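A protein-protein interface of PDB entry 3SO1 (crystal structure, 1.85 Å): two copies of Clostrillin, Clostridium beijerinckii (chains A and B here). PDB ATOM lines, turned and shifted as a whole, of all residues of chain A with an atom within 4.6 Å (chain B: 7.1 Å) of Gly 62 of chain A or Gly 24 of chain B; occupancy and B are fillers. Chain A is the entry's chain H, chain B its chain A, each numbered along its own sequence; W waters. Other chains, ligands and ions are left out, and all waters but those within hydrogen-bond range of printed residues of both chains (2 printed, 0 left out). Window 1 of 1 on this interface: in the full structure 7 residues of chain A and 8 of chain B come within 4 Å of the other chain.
Of the printed residues of chain B, Asn 57 of chain A touches Gln 30. Of the printed residues of chain B, Thr 61 of chain A touches Asn 25 (3.2 Å), Thr 27 (3.9 Å) and Gln 30 (2.8 Å). Gly 62 of chain A touches just these residues of chain B: Gly 24 (3.3 Å), Asn 25 (2.8 Å), Tyr 26 (3.7 Å) and Gln 30 (3.2 Å). Of the printed residues of chain A, Pro 23 of chain B touches Thr 63 (3.4 Å) and Lys 64 (2.8 Å). Gly 24 of chain B touches two residues of chain A. Printed residues of chain A within 4 Å of Gln 30 of chain B: Asn 57 (3.1 Å), Thr 61 (2.8 Å) and Gly 62 (3.2 Å). Val 85 of chain B touches none of the printed residues of chain A. Ile 87 of chain B touches none of the printed residues of chain A. The nearest residue of chain B that does not touch Gly 62 of chain A is Pro 23 of chain B (4.6 Å).
NE2 of Gln 30 of chain B is in hydrogen-bond range of OG1 of Thr 61 of chain A (2.8 Å). OG1 of Thr 63 of chain A sits at hydrogen-bond distance from OH of Tyr 26 of chain B (3.0 Å). The side-chain amide oxygen (OE1) of Gln 30 of chain B is in hydrogen-bond range of the backbone NH (N) of Gly 62 of chain A, at 3.2 Å. The side-chain amide nitrogen (ND2) of Asn 57 of chain A lies close to the side-chain amide nitrogen (NE2) of Gln 30 of chain B. N of Gly 62 of chain A is in hydrogen-bond range of O of Asn 25 of chain B. N of Lys 64 of chain A lies within hydrogen-bond range of O of Pro 23 of chain B (2.8 Å).
No position is printed for both chains. Of the 15 pairs that touch across the chains among the printed residues, none has its exchanged pair printed and touching as well.
Water W1 lies within hydrogen-bond range of the side-chain amino group of Lys 64 of chain A (2.7 Å), the side-chain amide oxygen of Asn 25 of chain B (2.9 Å) and the backbone carbonyl oxygen of Ile 87 of chain B (2.9 Å). Water W2 lies within hydrogen-bond range of N of Ser 89 of chain B (2.9 Å) and NZ of Lys 64 of chain A (3.3 Å).
The backbone carbonyl oxygen (O) of Gln 22 of chain B lies within hydrogen-bond range of the side-chain hydroxyl (OH) of Tyr 26 of chain B (2.6 Å). The backbone carbonyl oxygen of Asn 25 of chain B lies close to the side-chain amide oxygen of Gln 30 of chain B (3.4 Å). The backbone NH of Glu 56 of chain A lies within hydrogen-bond range of the backbone carbonyl oxygen of Thr 63 of chain A (2.8 Å). The side-chain amide oxygen of Gln 30 of chain B lies within hydrogen-bond range of the backbone NH of Thr 27 of chain B (3.0 Å). The backbone carbonyl oxygen of Val 85 of chain B sits at hydrogen-bond distance from the backbone NH of Tyr 26 of chain B (2.8 Å). The side-chain hydroxyl (OH) of Tyr 26 of chain B sits at hydrogen-bond distance from the backbone carbonyl oxygen (O) of Pro 23 of chain B (3.5 Å).
Of the 7 printed residues of chain A, 6 touch a printed residue of chain B. Hydrophobic or aromatic side chains of chain A that line the printed part of chain B: Tyr 55. Hydrophobic or aromatic side chains of chain B that line the printed part of chain A: Tyr 26 and Tyr 88. Among the printed residues, 15 pairs touch across the chains.
Among the printed residues, merely in contact across the chains: Thr 61 of chain A with Asn 25 of chain B (3.2 Å), Gly 62 of chain A with Gly 24 of chain B (3.3 Å), Tyr 55 of chain A with Asn 25 of chain B (3.4 Å), Thr 63 of chain A with Pro 23 of chain B (3.4 Å), Lys 64 of chain A with Tyr 88 of chain B (3.6 Å), Lys 64 of chain A with Gly 24 of chain B (3.6 Å), Gly 62 of chain A with Tyr 26 of chain B (3.7 Å), Thr 63 of chain A with Gln 22 of chain B (3.8 Å) and Thr 61 of chain A with Thr 27 of chain B (3.9 Å).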
ATOM      1  N   TYR A  55     -21.130   6.630  12.939  1.00  0.00           N
ATOM      2  CA  TYR A  55     -19.687   6.435  12.840  1.00  0.00           C
ATOM      3  C   TYR A  55     -19.278   4.977  12.977  1.00  0.00           C
ATOM      4  O   TYR A  55     -19.786   4.246  13.833  1.00  0.00           O
ATOM      5  CB  TYR A  55     -18.954   7.268  13.885  1.00  0.00           C
ATOM      6  CG  TYR A  55     -19.070   8.760  13.693  1.00  0.00           C
ATOM      7  CD1 TYR A  55     -20.107   9.479  14.288  1.00  0.00           C
ATOM      8  CD2 TYR A  55     -18.132   9.457  12.936  1.00  0.00           C
ATOM      9  CE1 TYR A  55     -20.211  10.850  14.129  1.00  0.00           C
ATOM     10  CE2 TYR A  55     -18.226  10.835  12.773  1.00  0.00           C
ATOM     11  CZ  TYR A  55     -19.269  11.523  13.371  1.00  0.00           C
ATOM     12  OH  TYR A  55     -19.370  12.887  13.209  1.00  0.00           O
ATOM     13  N   GLU A  56     -18.337   4.582  12.128  1.00  0.00           N
ATOM     14  CA  GLU A  56     -17.815   3.222  12.078  1.00  0.00           C
ATOM     15  C   GLU A  56     -17.132   2.832  13.386  1.00  0.00           C
ATOM     16  O   GLU A  56     -17.268   1.703  13.856  1.00  0.00           O
ATOM     17  CB  GLU A  56     -16.833   3.112  10.910  1.00  0.00           C
ATOM     18  CG  GLU A  56     -16.087   1.794  10.804  1.00  0.00           C
ATOM     19  CD  GLU A  56     -14.860   1.886   9.907  1.00  0.00           C
ATOM     20  OE1 GLU A  56     -14.290   2.998   9.746  1.00  0.00           O
ATOM     21  OE2 GLU A  56     -14.456   0.831   9.372  1.00  0.00           O
ATOM     22  N   ASN A  57     -16.397   3.772  13.967  1.00  0.00           N
ATOM     23  CA  ASN A  57     -15.658   3.510  15.192  1.00  0.00           C
ATOM     24  C   ASN A  57     -16.217   4.316  16.359  1.00  0.00           C
ATOM     25  O   ASN A  57     -17.101   5.161  16.174  1.00  0.00           O
ATOM     26  CB  ASN A  57     -14.167   3.795  14.984  1.00  0.00           C
ATOM     27  CG  ASN A  57     -13.527   2.858  13.970  1.00  0.00           C
ATOM     28  OD1 ASN A  57     -13.737   1.641  14.001  1.00  0.00           O
ATOM     29  ND2 ASN A  57     -12.736   3.423  13.070  1.00  0.00           N
ATOM     30  N   THR A  61     -15.345   8.707  15.289  1.00  0.00           N
ATOM     31  CA  THR A  61     -14.235   8.589  14.348  1.00  0.00           C
ATOM     32  C   THR A  61     -14.467   7.429  13.377  1.00  0.00           C
ATOM     33  O   THR A  61     -15.431   6.670  13.517  1.00  0.00           O
ATOM     34  CB  THR A  61     -12.868   8.426  15.065  1.00  0.00           C
ATOM     35  OG1 THR A  61     -12.912   7.297  15.944  1.00  0.00           O
ATOM     36  CG2 THR A  61     -12.495   9.698  15.849  1.00  0.00           C
ATOM     37  N   GLY A  62     -13.576   7.299  12.397  1.00  0.00           N
ATOM     38  CA  GLY A  62     -13.752   6.332  11.316  1.00  0.00           C
ATOM     39  C   GLY A  62     -14.755   6.868  10.310  1.00  0.00           C
ATOM     40  O   GLY A  62     -15.141   8.039  10.376  1.00  0.00           O
ATOM     41  N   THR A  63     -15.177   6.017   9.378  1.00  0.00           N
ATOM     42  CA  THR A  63     -16.140   6.410   8.344  1.00  0.00           C
ATOM     43  C   THR A  63     -17.438   6.919   8.965  1.00  0.00           C
ATOM     44  O   THR A  63     -17.917   6.368   9.957  1.00  0.00           O
ATOM     45  CB  THR A  63     -16.448   5.232   7.398  1.00  0.00           C
ATOM     46  OG1 THR A  63     -15.219   4.716   6.881  1.00  0.00           O
ATOM     47  CG2 THR A  63     -17.338   5.674   6.235  1.00  0.00           C
ATOM     48  N   LYS A  64     -17.986   7.974   8.371  1.00  0.00           N
ATOM     49  CA  LYS A  64     -19.216   8.596   8.837  1.00  0.00           C
ATOM     50  C   LYS A  64     -20.305   8.501   7.764  1.00  0.00           C
ATOM     51  O   LYS A  64     -20.109   8.944   6.636  1.00  0.00           O
ATOM     52  CB  LYS A  64     -18.942  10.058   9.203  1.00  0.00           C
ATOM     53  CG  LYS A  64     -20.143  10.847   9.689  1.00  0.00           C
ATOM     54  CD  LYS A  64     -19.810  12.337   9.794  1.00  0.00           C
ATOM     55  CE  LYS A  64     -19.861  13.039   8.434  1.00  0.00           C
ATOM     56  NZ  LYS A  64     -19.199  14.385   8.480  1.00  0.00           N
ATOM     57  N   LEU B  21     -10.658   6.755   0.745  1.00  0.00           N
ATOM     58  CA  LEU B  21     -11.495   6.814   1.940  1.00  0.00           C
ATOM     59  C   LEU B  21     -12.807   7.563   1.697  1.00  0.00           C
ATOM     60  O   LEU B  21     -12.856   8.530   0.929  1.00  0.00           O
ATOM     61  CB  LEU B  21     -10.731   7.465   3.102  1.00  0.00           C
ATOM     62  CG  LEU B  21      -9.570   6.715   3.764  1.00  0.00           C
ATOM     63  CD1 LEU B  21      -9.084   7.509   4.965  1.00  0.00           C
ATOM     64  CD2 LEU B  21      -9.968   5.305   4.192  1.00  0.00           C
ATOM     65  N   GLN B  22     -13.861   7.097   2.366  1.00  0.00           N
ATOM     66  CA  GLN B  22     -15.166   7.757   2.380  1.00  0.00           C
ATOM     67  C   GLN B  22     -15.185   8.874   3.427  1.00  0.00           C
ATOM     68  O   GLN B  22     -14.270   8.960   4.249  1.00  0.00           O
ATOM     69  CB  GLN B  22     -16.264   6.731   2.694  1.00  0.00           C
ATOM     70  CG  GLN B  22     -16.529   5.737   1.574  1.00  0.00           C
ATOM     71  CD  GLN B  22     -16.941   6.430   0.297  1.00  0.00           C
ATOM     72  OE1 GLN B  22     -18.015   7.029   0.219  1.00  0.00           O
ATOM     73  NE2 GLN B  22     -16.079   6.368  -0.712  1.00  0.00           N
ATOM     74  N   PRO B  23     -16.224   9.735   3.409  1.00  0.00           N
ATOM     75  CA  PRO B  23     -16.327  10.751   4.456  1.00  0.00           C
ATOM     76  C   PRO B  23     -16.210  10.166   5.862  1.00  0.00           C
ATOM     77  O   PRO B  23     -16.656   9.041   6.118  1.00  0.00           O
ATOM     78  CB  PRO B  23     -17.720  11.335   4.238  1.00  0.00           C
ATOM     79  CG  PRO B  23     -17.925  11.216   2.765  1.00  0.00           C
ATOM     80  CD  PRO B  23     -17.289   9.890   2.397  1.00  0.00           C
ATOM     81  N   GLY B  24     -15.598  10.932   6.759  1.00  0.00           N
ATOM     82  CA  GLY B  24     -15.363  10.478   8.124  1.00  0.00           C
ATOM     83  C   GLY B  24     -14.205  11.204   8.778  1.00  0.00           C
ATOM     84  O   GLY B  24     -13.557  12.052   8.158  1.00  0.00           O
ATOM     85  N   ASN B  25     -13.951  10.858  10.039  1.00  0.00           N
ATOM     86  CA  ASN B  25     -12.917  11.497  10.843  1.00  0.00           C
ATOM     87  C   ASN B  25     -11.903  10.447  11.266  1.00  0.00           C
ATOM     88  O   ASN B  25     -12.161   9.659  12.175  1.00  0.00           O
ATOM     89  CB  ASN B  25     -13.535  12.159  12.082  1.00  0.00           C
ATOM     90  CG  ASN B  25     -14.681  13.103  11.743  1.00  0.00           C
ATOM     91  OD1 ASN B  25     -14.652  13.816  10.738  1.00  0.00           O
ATOM     92  ND2 ASN B  25     -15.695  13.121  12.600  1.00  0.00           N
ATOM     93  N   TYR B  26     -10.753  10.441  10.605  1.00  0.00           N
ATOM     94  CA  TYR B  26      -9.801   9.352  10.746  1.00  0.00           C
ATOM     95  C   TYR B  26      -8.593   9.725  11.593  1.00  0.00           C
ATOM     96  O   TYR B  26      -7.852  10.647  11.255  1.00  0.00           O
ATOM     97  CB  TYR B  26      -9.365   8.865   9.358  1.00  0.00           C
ATOM     98  CG  TYR B  26     -10.522   8.410   8.493  1.00  0.00           C
ATOM     99  CD1 TYR B  26     -11.176   9.305   7.643  1.00  0.00           C
ATOM    100  CD2 TYR B  26     -10.971   7.088   8.534  1.00  0.00           C
ATOM    101  CE1 TYR B  26     -12.249   8.890   6.845  1.00  0.00           C
ATOM    102  CE2 TYR B  26     -12.042   6.664   7.737  1.00  0.00           C
ATOM    103  CZ  TYR B  26     -12.672   7.572   6.895  1.00  0.00           C
ATOM    104  OH  TYR B  26     -13.728   7.158   6.106  1.00  0.00           O
ATOM    105  N   THR B  27      -8.405   8.992  12.691  1.00  0.00           N
ATOM    106  CA  THR B  27      -7.230   9.150  13.548  1.00  0.00           C
ATOM    107  C   THR B  27      -6.019   8.449  12.926  1.00  0.00           C
ATOM    108  O   THR B  27      -6.158   7.707  11.949  1.00  0.00           O
ATOM    109  CB  THR B  27      -7.457   8.545  14.949  1.00  0.00           C
ATOM    110  OG1 THR B  27      -7.663   7.132  14.825  1.00  0.00           O
ATOM    111  CG2 THR B  27      -8.674   9.182  15.631  1.00  0.00           C
ATOM    112  N   GLN B  30      -6.337   4.707  12.804  1.00  0.00           N
ATOM    113  CA  GLN B  30      -7.338   4.351  11.789  1.00  0.00           C
ATOM    114  C   GLN B  30      -6.792   4.484  10.358  1.00  0.00           C
ATOM    115  O   GLN B  30      -7.074   3.642   9.499  1.00  0.00           O
ATOM    116  CB  GLN B  30      -8.616   5.167  11.995  1.00  0.00           C
ATOM    117  CG  GLN B  30      -9.371   4.771  13.261  1.00  0.00           C
ATOM    118  CD  GLN B  30     -10.355   5.823  13.740  1.00  0.00           C
ATOM    119  OE1 GLN B  30     -10.448   6.919  13.183  1.00  0.00           O
ATOM    120  NE2 GLN B  30     -11.099   5.488  14.785  1.00  0.00           N
ATOM    121  N   PHE B  60      -6.875  15.288  15.130  1.00  0.00           N
ATOM    122  CA  PHE B  60      -7.352  16.535  14.520  1.00  0.00           C
ATOM    123  C   PHE B  60      -6.830  17.768  15.268  1.00  0.00           C
ATOM    124  O   PHE B  60      -7.580  18.695  15.597  1.00  0.00           O
ATOM    125  CB  PHE B  60      -8.885  16.496  14.382  1.00  0.00           C
ATOM    126  CG  PHE B  60      -9.411  15.107  14.139  1.00  0.00           C
ATOM    127  CD1 PHE B  60     -10.048  14.401  15.154  1.00  0.00           C
ATOM    128  CD2 PHE B  60      -9.188  14.473  12.917  1.00  0.00           C
ATOM    129  CE1 PHE B  60     -10.495  13.097  14.945  1.00  0.00           C
ATOM    130  CE2 PHE B  60      -9.636  13.171  12.694  1.00  0.00           C
ATOM    131  CZ  PHE B  60     -10.288  12.483  13.707  1.00  0.00           C
ATOM    132  N   VAL B  85      -7.144  13.149   9.695  1.00  0.00           N
ATOM    133  CA  VAL B  85      -7.865  13.795   8.600  1.00  0.00           C
ATOM    134  C   VAL B  85      -9.380  13.705   8.769  1.00  0.00           C
ATOM    135  O   VAL B  85      -9.917  12.666   9.171  1.00  0.00           O
ATOM    136  CB  VAL B  85      -7.392  13.240   7.210  1.00  0.00           C
ATOM    137  CG1 VAL B  85      -7.769  11.768   7.032  1.00  0.00           C
ATOM    138  CG2 VAL B  85      -7.931  14.082   6.062  1.00  0.00           C
ATOM    139  N   LYS B  86     -10.058  14.815   8.489  1.00  0.00           N
ATOM    140  CA  LYS B  86     -11.516  14.837   8.440  1.00  0.00           C
ATOM    141  C   LYS B  86     -11.982  15.051   7.003  1.00  0.00           C
ATOM    142  O   LYS B  86     -11.546  15.989   6.336  1.00  0.00           O
ATOM    143  CB  LYS B  86     -12.076  15.922   9.360  1.00  0.00           C
ATOM    144  CG  LYS B  86     -11.916  15.607  10.841  1.00  0.00           C
ATOM    145  CD  LYS B  86     -12.612  16.647  11.706  1.00  0.00           C
ATOM    146  CE  LYS B  86     -12.556  16.269  13.173  1.00  0.00           C
ATOM    147  NZ  LYS B  86     -13.130  17.357  14.027  1.00  0.00           N
ATOM    148  N   ILE B  87     -12.845  14.155   6.535  1.00  0.00           N
ATOM    149  CA  ILE B  87     -13.375  14.196   5.172  1.00  0.00           C
ATOM    150  C   ILE B  87     -14.880  14.458   5.230  1.00  0.00           C
ATOM    151  O   ILE B  87     -15.617  13.720   5.886  1.00  0.00           O
ATOM    152  CB  ILE B  87     -13.087  12.877   4.399  1.00  0.00           C
ATOM    153  CG1 ILE B  87     -11.577  12.610   4.309  1.00  0.00           C
ATOM    154  CG2 ILE B  87     -13.713  12.918   3.007  1.00  0.00           C
ATOM    155  CD1 ILE B  87     -11.212  11.183   3.869  1.00  0.00           C
ATOM    156  N   TYR B  88     -15.311  15.517   4.540  1.00  0.00           N
ATOM    157  CA  TYR B  88     -16.712  15.937   4.483  1.00  0.00           C
ATOM    158  C   TYR B  88     -17.209  15.938   3.041  1.00  0.00           C
ATOM    159  O   TYR B  88     -16.507  16.411   2.147  1.00  0.00           O
ATOM    160  CB  TYR B  88     -16.866  17.360   5.025  1.00  0.00           C
ATOM    161  CG  TYR B  88     -16.458  17.553   6.462  1.00  0.00           C
ATOM    162  CD1 TYR B  88     -15.189  18.028   6.790  1.00  0.00           C
ATOM    163  CD2 TYR B  88     -17.349  17.278   7.498  1.00  0.00           C
ATOM    164  CE1 TYR B  88     -14.811  18.220   8.119  1.00  0.00           C
ATOM    165  CE2 TYR B  88     -16.983  17.463   8.831  1.00  0.00           C
ATOM    166  CZ  TYR B  88     -15.715  17.934   9.131  1.00  0.00           C
ATOM    167  OH  TYR B  88     -15.359  18.114  10.447  1.00  0.00           O
ATOM    168  N   SER B  89     -18.418  15.427   2.816  1.00  0.00           N
ATOM    169  CA  SER B  89     -19.009  15.429   1.470  1.00  0.00           C
ATOM    170  C   SER B  89     -19.611  16.793   1.078  1.00  0.00           C
ATOM    171  O   SER B  89     -20.299  16.909   0.052  1.00  0.00           O
ATOM    172  CB  SER B  89     -20.041  14.306   1.326  1.00  0.00           C
ATOM    173  OG  SER B  89     -21.088  14.450   2.268  1.00  0.00           O
HETATM  174  O   HOH W   1     -16.588  13.759   8.625  1.00  0.00           O
HETATM  175  O   HOH W   2     -19.745  14.508   5.237  1.00  0.00           O
